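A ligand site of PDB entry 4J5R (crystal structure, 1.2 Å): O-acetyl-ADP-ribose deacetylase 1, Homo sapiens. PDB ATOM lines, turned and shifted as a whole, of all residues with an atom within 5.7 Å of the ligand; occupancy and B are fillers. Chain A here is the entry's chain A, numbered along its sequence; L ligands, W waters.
An oxygen (O8) of the ligand sits at hydrogen-bond distance from the backbone NH (N) of Asp 119 (3.0 Å). N of Cys 116 lies within hydrogen-bond range of O8 of the ligand (3.4 Å). N of Gly 117 lies within hydrogen-bond range of O8 of the ligand (2.8 Å). O12 of the ligand is in hydrogen-bond range of NZ of Lys 78 (3.0 Å). An oxygen (O9) of the ligand is in hydrogen-bond range of the backbone NH (N) of Gly 115 (2.8 Å). The backbone NH (N) of Leu 118 sits at hydrogen-bond distance from an oxygen (O6) of the ligand. N of Ile 38 sits at hydrogen-bond distance from O5 of the ligand.
The backbone carbonyl oxygen (O) of Leu 118 lies close to the guanidinium group (NE) of Arg 120 (3.5 Å). The backbone carbonyl oxygen (O) of Gly 115 sits at hydrogen-bond distance from the backbone NH (N) of Arg 120, 3.3 Å away. The side-chain amino group (NZ) of Lys 78 lies within salt-bridge range of the side-chain carboxylate (OD1) of Asp 119 (2.8 Å). O of Gly 117 sits at hydrogen-bond distance from NH1 of Arg 120, 3.4 Å away. SG of Cys 116 is in hydrogen-bond range of O of Ile 114 (3.4 Å). The backbone NH (N) of Ala 81 lies within hydrogen-bond range of the side-chain hydroxyl (OG) of Ser 29. The side-chain amino group of Lys 78 sits at hydrogen-bond distance from the backbone carbonyl oxygen of Ala 81, at 2.8 Å.
Cys 27 touches the ligand (O to C13, 3.4 Å). Ile 28 touches the ligand. Met 34 touches the ligand (CA to O11, 3.6 Å). Ala 36 touches the ligand (O to C12, 3.6 Å). Gly 37 touches the ligand (C to N4, 3.4 Å). CB of Ala 39 touches O11 of the ligand (3.4 Å). CD1 of Leu 41 touches N3 of the ligand, at 3.4 Å. Ala 81 touches the ligand (O to O12, 3.8 Å). Pro 112 touches the ligand. O of Arg 113 touches C10 of the ligand (3.4 Å). Leu 146 touches the ligand (CD1 to C1, 3.4 Å). Hydrophobic or aromatic side chains within 4 Å of the ligand: Ile 28, Ile 38, Ala 39, Leu 41, Pro 112, Leu 118 and Leu 146. The nearest printed residue that does not touch the ligand is Ile 114 (4.005 Å).
Water W5 lies within hydrogen-bond range of an oxygen (O9) of the ligand (2.8 Å) and the backbone NH of Cys 27 (2.9 Å). Water W9 lies within hydrogen-bond range of O5 of the ligand (2.8 Å), N of Ala 39 (3.0 Å), O of Ala 36 (3.3 Å) and N of Ile 38 (3.3 Å). Water W1 lies within hydrogen-bond range of the backbone carbonyl oxygen (O) of Gly 37 (2.8 Å) and a nitrogen (N3) of the ligand (2.9 Å). Water W10 lies within hydrogen-bond range of O2 of the ligand and O of Cys 116. Water W3 lies within hydrogen-bond range of the backbone NH of Leu 146 (2.8 Å) and a nitrogen (N2) of the ligand (3.1 Å). Water W4 lies within hydrogen-bond range of the side-chain carboxylate (OD2) of Asp 119 (2.8 Å) and the backbone carbonyl oxygen (O) of Ile 28 (3.2 Å).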
ATOM      1  N   CYS A  27     -15.981  23.605  -6.800  1.00  0.00           N
ATOM      2  CA  CYS A  27     -15.774  22.186  -7.122  1.00  0.00           C
ATOM      3  C   CYS A  27     -16.613  21.259  -6.244  1.00  0.00           C
ATOM      4  O   CYS A  27     -16.615  21.432  -5.009  1.00  0.00           O
ATOM      5  CB  CYS A  27     -14.338  21.771  -6.965  1.00  0.00           C
ATOM      6  SG  CYS A  27     -13.164  22.714  -7.968  1.00  0.00           S
ATOM      7  N   ILE A  28     -17.231  20.241  -6.839  1.00  0.00           N
ATOM      8  CA  ILE A  28     -17.952  19.230  -6.107  1.00  0.00           C
ATOM      9  C   ILE A  28     -17.701  17.868  -6.747  1.00  0.00           C
ATOM     10  O   ILE A  28     -17.037  17.748  -7.784  1.00  0.00           O
ATOM     11  CB  ILE A  28     -19.476  19.544  -6.055  1.00  0.00           C
ATOM     12  CG1 ILE A  28     -20.112  19.425  -7.467  1.00  0.00           C
ATOM     13  CG2 ILE A  28     -19.716  20.908  -5.432  1.00  0.00           C
ATOM     14  CD1 ILE A  28     -21.616  19.236  -7.407  1.00  0.00           C
ATOM     15  N   SER A  29     -18.270  16.821  -6.138  1.00  0.00           N
ATOM     16  CA  SER A  29     -18.263  15.479  -6.700  1.00  0.00           C
ATOM     17  C   SER A  29     -19.517  15.153  -7.457  1.00  0.00           C
ATOM     18  O   SER A  29     -20.543  15.835  -7.327  1.00  0.00           O
ATOM     19  CB  SER A  29     -18.054  14.398  -5.643  1.00  0.00           C
ATOM     20  OG  SER A  29     -19.251  14.062  -4.934  1.00  0.00           O
ATOM     21  N   ARG A  33     -23.124  16.035  -2.762  1.00  0.00           N
ATOM     22  CA  ARG A  33     -23.399  16.098  -1.324  1.00  0.00           C
ATOM     23  C   ARG A  33     -23.117  17.501  -0.748  1.00  0.00           C
ATOM     24  O   ARG A  33     -23.831  17.962   0.144  1.00  0.00           O
ATOM     25  CB  ARG A  33     -22.622  15.018  -0.559  1.00  0.00           C
ATOM     26  CG  ARG A  33     -23.162  13.634  -0.901  1.00  0.00           C
ATOM     27  CD  ARG A  33     -22.355  12.441  -0.407  1.00  0.00           C
ATOM     28  NE  ARG A  33     -22.368  12.305   1.044  1.00  0.00           N
ATOM     29  CZ  ARG A  33     -21.474  11.572   1.741  1.00  0.00           C
ATOM     30  NH1 ARG A  33     -20.454  10.987   1.149  1.00  0.00           N
ATOM     31  NH2 ARG A  33     -21.561  11.473   3.046  1.00  0.00           N
ATOM     32  N   MET A  34     -22.052  18.118  -1.177  1.00  0.00           N
ATOM     33  CA  MET A  34     -21.731  19.508  -0.813  1.00  0.00           C
ATOM     34  C   MET A  34     -21.802  19.738   0.700  1.00  0.00           C
ATOM     35  O   MET A  34     -22.450  20.660   1.177  1.00  0.00           O
ATOM     36  CB  MET A  34     -22.613  20.477  -1.567  1.00  0.00           C
ATOM     37  CG  MET A  34     -22.444  20.366  -3.072  1.00  0.00           C
ATOM     38  SD  MET A  34     -23.188  21.744  -3.993  1.00  0.00           S
ATOM     39  CE  MET A  34     -24.897  21.379  -3.881  1.00  0.00           C
ATOM     40  N   GLY A  35     -21.122  18.890   1.472  1.00  0.00           N
ATOM     41  CA  GLY A  35     -21.298  18.879   2.916  1.00  0.00           C
ATOM     42  C   GLY A  35     -20.291  19.657   3.747  1.00  0.00           C
ATOM     43  O   GLY A  35     -20.415  19.708   4.971  1.00  0.00           O
ATOM     44  N   ALA A  36     -19.274  20.189   3.073  1.00  0.00           N
ATOM     45  CA  ALA A  36     -18.169  20.817   3.741  1.00  0.00           C
ATOM     46  C   ALA A  36     -17.627  21.974   2.938  1.00  0.00           C
ATOM     47  O   ALA A  36     -18.058  22.210   1.790  1.00  0.00           O
ATOM     48  CB  ALA A  36     -17.100  19.778   4.042  1.00  0.00           C
ATOM     49  N   GLY A  37     -16.632  22.672   3.464  1.00  0.00           N
ATOM     50  CA  GLY A  37     -15.975  23.720   2.743  1.00  0.00           C
ATOM     51  C   GLY A  37     -16.900  24.822   2.323  1.00  0.00           C
ATOM     52  O   GLY A  37     -17.959  25.052   2.924  1.00  0.00           O
ATOM     53  N   ILE A  38     -16.577  25.483   1.236  1.00  0.00           N
ATOM     54  CA  ILE A  38     -17.459  26.483   0.659  1.00  0.00           C
ATOM     55  C   ILE A  38     -18.689  25.817   0.031  1.00  0.00           C
ATOM     56  O   ILE A  38     -19.731  26.467  -0.120  1.00  0.00           O
ATOM     57  CB  ILE A  38     -16.699  27.373  -0.326  1.00  0.00           C
ATOM     58  CG1 ILE A  38     -17.446  28.697  -0.473  1.00  0.00           C
ATOM     59  CG2 ILE A  38     -16.493  26.680  -1.654  1.00  0.00           C
ATOM     60  CD1 ILE A  38     -16.708  29.732  -1.239  1.00  0.00           C
ATOM     61  N   ALA A  39     -18.596  24.533  -0.312  1.00  0.00           N
ATOM     62  CA  ALA A  39     -19.715  23.921  -0.987  1.00  0.00           C
ATOM     63  C   ALA A  39     -20.965  23.938  -0.167  1.00  0.00           C
ATOM     64  O   ALA A  39     -22.064  24.111  -0.701  1.00  0.00           O
ATOM     65  CB  ALA A  39     -19.381  22.495  -1.432  1.00  0.00           C
ATOM     66  N   LEU A  41     -21.977  26.091   1.817  1.00  0.00           N
ATOM     67  CA  LEU A  41     -22.524  27.429   1.674  1.00  0.00           C
ATOM     68  C   LEU A  41     -23.210  27.659   0.340  1.00  0.00           C
ATOM     69  O   LEU A  41     -24.265  28.307   0.299  1.00  0.00           O
ATOM     70  CB  LEU A  41     -21.434  28.495   1.947  1.00  0.00           C
ATOM     71  CG  LEU A  41     -20.793  28.412   3.346  1.00  0.00           C
ATOM     72  CD1 LEU A  41     -19.781  29.533   3.494  1.00  0.00           C
ATOM     73  CD2 LEU A  41     -21.838  28.483   4.432  1.00  0.00           C
ATOM     74  N   LYS A  78     -14.526  14.934  -9.522  1.00  0.00           N
ATOM     75  CA  LYS A  78     -14.265  13.637  -8.904  1.00  0.00           C
ATOM     76  C   LYS A  78     -15.573  12.890  -8.734  1.00  0.00           C
ATOM     77  O   LYS A  78     -16.653  13.499  -8.805  1.00  0.00           O
ATOM     78  CB  LYS A  78     -13.526  13.828  -7.554  1.00  0.00           C
ATOM     79  CG  LYS A  78     -14.374  14.475  -6.518  1.00  0.00           C
ATOM     80  CD  LYS A  78     -13.625  14.991  -5.324  1.00  0.00           C
ATOM     81  CE  LYS A  78     -14.556  15.345  -4.218  1.00  0.00           C
ATOM     82  NZ  LYS A  78     -13.854  15.788  -2.976  1.00  0.00           N
ATOM     83  N   ARG A  80     -16.666  10.554  -5.969  1.00  0.00           N
ATOM     84  CA  ARG A  80     -17.268  10.504  -4.628  1.00  0.00           C
ATOM     85  C   ARG A  80     -16.794  11.693  -3.816  1.00  0.00           C
ATOM     86  O   ARG A  80     -15.684  12.201  -4.039  1.00  0.00           O
ATOM     87  CB  ARG A  80     -16.833   9.231  -3.883  1.00  0.00           C
ATOM     88  CG  ARG A  80     -17.107   7.865  -4.532  1.00  0.00           C
ATOM     89  CD  ARG A  80     -18.469   7.319  -4.286  1.00  0.00           C
ATOM     90  NE  ARG A  80     -19.367   7.990  -5.200  1.00  0.00           N
ATOM     91  CZ  ARG A  80     -19.642   7.628  -6.463  1.00  0.00           C
ATOM     92  NH1 ARG A  80     -19.070   6.541  -7.044  1.00  0.00           N
ATOM     93  NH2 ARG A  80     -20.489   8.412  -7.163  1.00  0.00           N
ATOM     94  N   ALA A  81     -17.592  12.103  -2.837  1.00  0.00           N
ATOM     95  CA  ALA A  81     -17.261  13.258  -2.018  1.00  0.00           C
ATOM     96  C   ALA A  81     -15.920  13.094  -1.339  1.00  0.00           C
ATOM     97  O   ALA A  81     -15.145  14.052  -1.204  1.00  0.00           O
ATOM     98  CB  ALA A  81     -18.360  13.512  -0.997  1.00  0.00           C
ATOM     99  N   PRO A 112     -13.753  30.747  -5.189  1.00  0.00           N
ATOM    100  CA  PRO A 112     -12.757  30.618  -4.153  1.00  0.00           C
ATOM    101  C   PRO A 112     -11.479  30.018  -4.779  1.00  0.00           C
ATOM    102  O   PRO A 112     -11.361  29.904  -5.999  1.00  0.00           O
ATOM    103  CB  PRO A 112     -13.444  29.641  -3.212  1.00  0.00           C
ATOM    104  CG  PRO A 112     -14.089  28.662  -4.145  1.00  0.00           C
ATOM    105  CD  PRO A 112     -14.618  29.548  -5.244  1.00  0.00           C
ATOM    106  N   ARG A 113     -10.511  29.657  -3.940  1.00  0.00           N
ATOM    107  CA  ARG A 113      -9.313  28.948  -4.378  1.00  0.00           C
ATOM    108  C   ARG A 113      -9.681  27.506  -4.657  1.00  0.00           C
ATOM    109  O   ARG A 113      -9.375  26.565  -3.882  1.00  0.00           O
ATOM    110  CB  ARG A 113      -8.157  29.080  -3.379  1.00  0.00           C
ATOM    111  CG  ARG A 113      -7.478  30.429  -3.399  1.00  0.00           C
ATOM    112  CD  ARG A 113      -6.198  30.401  -2.595  1.00  0.00           C
ATOM    113  NE  ARG A 113      -5.471  31.657  -2.687  1.00  0.00           N
ATOM    114  CZ  ARG A 113      -4.179  31.787  -2.435  1.00  0.00           C
ATOM    115  NH1 ARG A 113      -3.486  30.739  -1.997  1.00  0.00           N
ATOM    116  NH2 ARG A 113      -3.609  32.971  -2.567  1.00  0.00           N
ATOM    117  N   ILE A 114     -10.389  27.314  -5.779  1.00  0.00           N
ATOM    118  CA  ILE A 114     -10.958  26.034  -6.120  1.00  0.00           C
ATOM    119  C   ILE A 114      -9.936  24.892  -6.123  1.00  0.00           C
ATOM    120  O   ILE A 114      -8.833  25.001  -6.625  1.00  0.00           O
ATOM    121  CB  ILE A 114     -11.626  26.150  -7.533  1.00  0.00           C
ATOM    122  CG1 ILE A 114     -10.684  26.724  -8.585  1.00  0.00           C
ATOM    123  CG2 ILE A 114     -12.930  26.925  -7.445  1.00  0.00           C
ATOM    124  CD1 ILE A 114     -11.144  26.477  -9.996  1.00  0.00           C
ATOM    125  N   GLY A 115     -10.348  23.760  -5.532  1.00  0.00           N
ATOM    126  CA  GLY A 115      -9.549  22.583  -5.472  1.00  0.00           C
ATOM    127  C   GLY A 115      -8.487  22.556  -4.365  1.00  0.00           C
ATOM    128  O   GLY A 115      -7.867  21.510  -4.146  1.00  0.00           O
ATOM    129  N   CYS A 116      -8.283  23.665  -3.683  1.00  0.00           N
ATOM    130  CA  CYS A 116      -7.060  23.878  -2.872  1.00  0.00           C
ATOM    131  C   CYS A 116      -7.370  23.924  -1.363  1.00  0.00           C
ATOM    132  O   CYS A 116      -6.500  24.294  -0.586  1.00  0.00           O
ATOM    133  CB  CYS A 116      -6.351  25.138  -3.300  1.00  0.00           C
ATOM    134  SG  CYS A 116      -5.775  24.995  -5.032  1.00  0.00           S
ATOM    135  N   GLY A 117      -8.587  23.541  -0.960  1.00  0.00           N
ATOM    136  CA  GLY A 117      -8.955  23.328   0.449  1.00  0.00           C
ATOM    137  C   GLY A 117      -8.926  21.835   0.715  1.00  0.00           C
ATOM    138  O   GLY A 117      -7.888  21.173   0.665  1.00  0.00           O
ATOM    139  N   LEU A 118     -10.098  21.297   0.959  1.00  0.00           N
ATOM    140  CA  LEU A 118     -10.258  19.873   1.177  1.00  0.00           C
ATOM    141  C   LEU A 118      -9.757  19.014   0.070  1.00  0.00           C
ATOM    142  O   LEU A 118      -9.319  17.893   0.292  1.00  0.00           O
ATOM    143  CB  LEU A 118     -11.730  19.520   1.511  1.00  0.00           C
ATOM    144  CG  LEU A 118     -12.173  20.023   2.894  1.00  0.00           C
ATOM    145  CD1 LEU A 118     -13.669  20.232   2.943  1.00  0.00           C
ATOM    146  CD2 LEU A 118     -11.696  19.073   3.969  1.00  0.00           C
ATOM    147  N   ASP A 119      -9.789  19.509  -1.171  1.00  0.00           N
ATOM    148  CA  ASP A 119      -9.359  18.706  -2.328  1.00  0.00           C
ATOM    149  C   ASP A 119      -7.854  18.625  -2.513  1.00  0.00           C
ATOM    150  O   ASP A 119      -7.398  17.845  -3.325  1.00  0.00           O
ATOM    151  CB  ASP A 119     -10.099  19.150  -3.596  1.00  0.00           C
ATOM    152  CG  ASP A 119     -11.459  18.570  -3.771  1.00  0.00           C
ATOM    153  OD1 ASP A 119     -11.919  17.746  -2.940  1.00  0.00           O
ATOM    154  OD2 ASP A 119     -12.101  18.906  -4.814  1.00  0.00           O
ATOM    155  N   ARG A 120      -7.106  19.382  -1.720  1.00  0.00           N
ATOM    156  CA  ARG A 120      -5.653  19.221  -1.569  1.00  0.00           C
ATOM    157  C   ARG A 120      -4.775  19.591  -2.757  1.00  0.00           C
ATOM    158  O   ARG A 120      -3.591  19.350  -2.736  1.00  0.00           O
ATOM    159  CB  ARG A 120      -5.240  17.785  -1.175  1.00  0.00           C
ATOM    160  CG  ARG A 120      -5.985  17.170  -0.067  1.00  0.00           C
ATOM    161  CD  ARG A 120      -5.934  18.011   1.180  1.00  0.00           C
ATOM    162  NE  ARG A 120      -6.559  17.265   2.280  1.00  0.00           N
ATOM    163  CZ  ARG A 120      -7.190  17.857   3.278  1.00  0.00           C
ATOM    164  NH1 ARG A 120      -7.178  19.190   3.385  1.00  0.00           N
ATOM    165  NH2 ARG A 120      -7.865  17.130   4.152  1.00  0.00           N
ATOM    166  N   TYR A 144     -11.664  34.821  -4.402  1.00  0.00           N
ATOM    167  CA  TYR A 144     -11.933  35.267  -3.001  1.00  0.00           C
ATOM    168  C   TYR A 144     -11.345  34.335  -2.000  1.00  0.00           C
ATOM    169  O   TYR A 144     -11.366  33.118  -2.173  1.00  0.00           O
ATOM    170  CB  TYR A 144     -13.417  35.301  -2.738  1.00  0.00           C
ATOM    171  CG  TYR A 144     -14.068  36.436  -3.401  1.00  0.00           C
ATOM    172  CD1 TYR A 144     -14.336  36.458  -4.746  1.00  0.00           C
ATOM    173  CD2 TYR A 144     -14.424  37.538  -2.667  1.00  0.00           C
ATOM    174  CE1 TYR A 144     -14.908  37.565  -5.353  1.00  0.00           C
ATOM    175  CE2 TYR A 144     -15.017  38.625  -3.253  1.00  0.00           C
ATOM    176  CZ  TYR A 144     -15.236  38.653  -4.592  1.00  0.00           C
ATOM    177  OH  TYR A 144     -15.803  39.752  -5.173  1.00  0.00           O
ATOM    178  N   THR A 145     -10.813  34.912  -0.918  1.00  0.00           N
ATOM    179  CA  THR A 145     -10.342  34.226   0.265  1.00  0.00           C
ATOM    180  C   THR A 145     -10.759  35.003   1.509  1.00  0.00           C
ATOM    181  O   THR A 145     -10.717  36.210   1.485  1.00  0.00           O
ATOM    182  CB  THR A 145      -8.826  34.289   0.261  1.00  0.00           C
ATOM    183  OG1 THR A 145      -8.374  35.656   0.352  1.00  0.00           O
ATOM    184  CG2 THR A 145      -8.315  33.712  -0.994  1.00  0.00           C
ATOM    185  N   LEU A 146     -11.063  34.331   2.619  1.00  0.00           N
ATOM    186  CA  LEU A 146     -11.461  35.029   3.856  1.00  0.00           C
ATOM    187  C   LEU A 146     -10.313  35.798   4.514  1.00  0.00           C
ATOM    188  O   LEU A 146      -9.129  35.395   4.452  1.00  0.00           O
ATOM    189  CB  LEU A 146     -12.091  34.045   4.842  1.00  0.00           C
ATOM    190  CG  LEU A 146     -13.432  33.433   4.432  1.00  0.00           C
ATOM    191  CD1 LEU A 146     -13.808  32.348   5.433  1.00  0.00           C
ATOM    192  CD2 LEU A 146     -14.548  34.475   4.348  1.00  0.00           C
ATOM    193  OXT LEU A 146     -10.622  36.843   5.119  1.00  0.00           O
HETATM  194  N1  LIG L   1     -16.005  30.213   3.689  1.00  0.00           N
HETATM  195  C1  LIG L   1     -15.148  30.768   2.771  1.00  0.00           C
HETATM  196  N2  LIG L   1     -14.123  30.048   2.195  1.00  0.00           N
HETATM  197  C2  LIG L   1     -14.091  28.798   2.645  1.00  0.00           C
HETATM  198  C3  LIG L   1     -14.926  28.155   3.500  1.00  0.00           C
HETATM  199  C4  LIG L   1     -15.924  28.928   4.002  1.00  0.00           C
HETATM  200  N3  LIG L   1     -16.849  28.459   4.956  1.00  0.00           N
HETATM  201  N4  LIG L   1     -14.555  26.869   3.647  1.00  0.00           N
HETATM  202  C5  LIG L   1     -13.535  26.682   2.840  1.00  0.00           C
HETATM  203  N5  LIG L   1     -13.189  27.842   2.258  1.00  0.00           N
HETATM  204  C6  LIG L   1     -12.083  28.030   1.309  1.00  0.00           C
HETATM  205  C7  LIG L   1     -10.812  27.203   1.547  1.00  0.00           C
HETATM  206  O1  LIG L   1     -10.056  27.699   2.604  1.00  0.00           O
HETATM  207  C8  LIG L   1     -10.224  27.410   0.245  1.00  0.00           C
HETATM  208  O2  LIG L   1      -9.329  28.383   0.092  1.00  0.00           O
HETATM  209  O3  LIG L   1     -12.458  27.747  -0.018  1.00  0.00           O
HETATM  210  C9  LIG L   1     -11.313  27.271  -0.726  1.00  0.00           C
HETATM  211  C10 LIG L   1     -11.615  25.921  -1.356  1.00  0.00           C
HETATM  212  O4  LIG L   1     -11.659  24.928  -0.349  1.00  0.00           O
HETATM  213  P1  LIG L   1     -12.903  23.910  -0.243  1.00  0.00           P
HETATM  214  O5  LIG L   1     -14.130  24.693   0.019  1.00  0.00           O
HETATM  215  O6  LIG L   1     -12.428  22.897   0.697  1.00  0.00           O
HETATM  216  O7  LIG L   1     -13.023  23.392  -1.751  1.00  0.00           O
HETATM  217  P2  LIG L   1     -12.194  22.268  -2.579  1.00  0.00           P
HETATM  218  O8  LIG L   1     -10.808  22.165  -2.066  1.00  0.00           O
HETATM  219  O9  LIG L   1     -12.459  22.628  -3.991  1.00  0.00           O
HETATM  220  O10 LIG L   1     -12.942  20.941  -2.178  1.00  0.00           O
HETATM  221  C11 LIG L   1     -14.188  20.593  -2.769  1.00  0.00           C
HETATM  222  N6  LIG L   1     -15.275  19.878  -0.647  1.00  0.00           N
HETATM  223  C12 LIG L   1     -16.748  19.892  -0.658  1.00  0.00           C
HETATM  224  O11 LIG L   1     -18.450  19.299  -2.295  1.00  0.00           O
HETATM  225  C13 LIG L   1     -17.127  19.739  -2.118  1.00  0.00           C
HETATM  226  O12 LIG L   1     -16.275  17.493  -2.270  1.00  0.00           O
HETATM  227  C14 LIG L   1     -16.048  18.864  -2.650  1.00  0.00           C
HETATM  228  C15 LIG L   1     -14.804  19.450  -2.020  1.00  0.00           C
HETATM  229  O   HOH W   1     -17.948  25.861   5.578  1.00  0.00           O
HETATM  230  O   HOH W   2      -7.971  25.812   3.316  1.00  0.00           O
HETATM  231  O   HOH W   3     -11.446  31.577   2.454  1.00  0.00           O
HETATM  232  O   HOH W   4     -14.666  18.380  -5.735  1.00  0.00           O
HETATM  233  O   HOH W   5     -14.267  24.606  -4.625  1.00  0.00           O
HETATM  234  O   HOH W   6      -8.772  31.092   0.742  1.00  0.00           O
HETATM  235  O   HOH W   7     -18.510  29.970   7.067  1.00  0.00           O
HETATM  236  O   HOH W   8     -17.879  32.265   4.327  1.00  0.00           O
HETATM  237  O   HOH W   9     -16.115  22.901  -0.827  1.00  0.00           O
HETATM  238  O   HOH W  10      -6.612  27.348   0.171  1.00  0.00           O
HETATM  239  O   HOH W  11     -10.807  30.692  -1.265  1.00  0.00           O
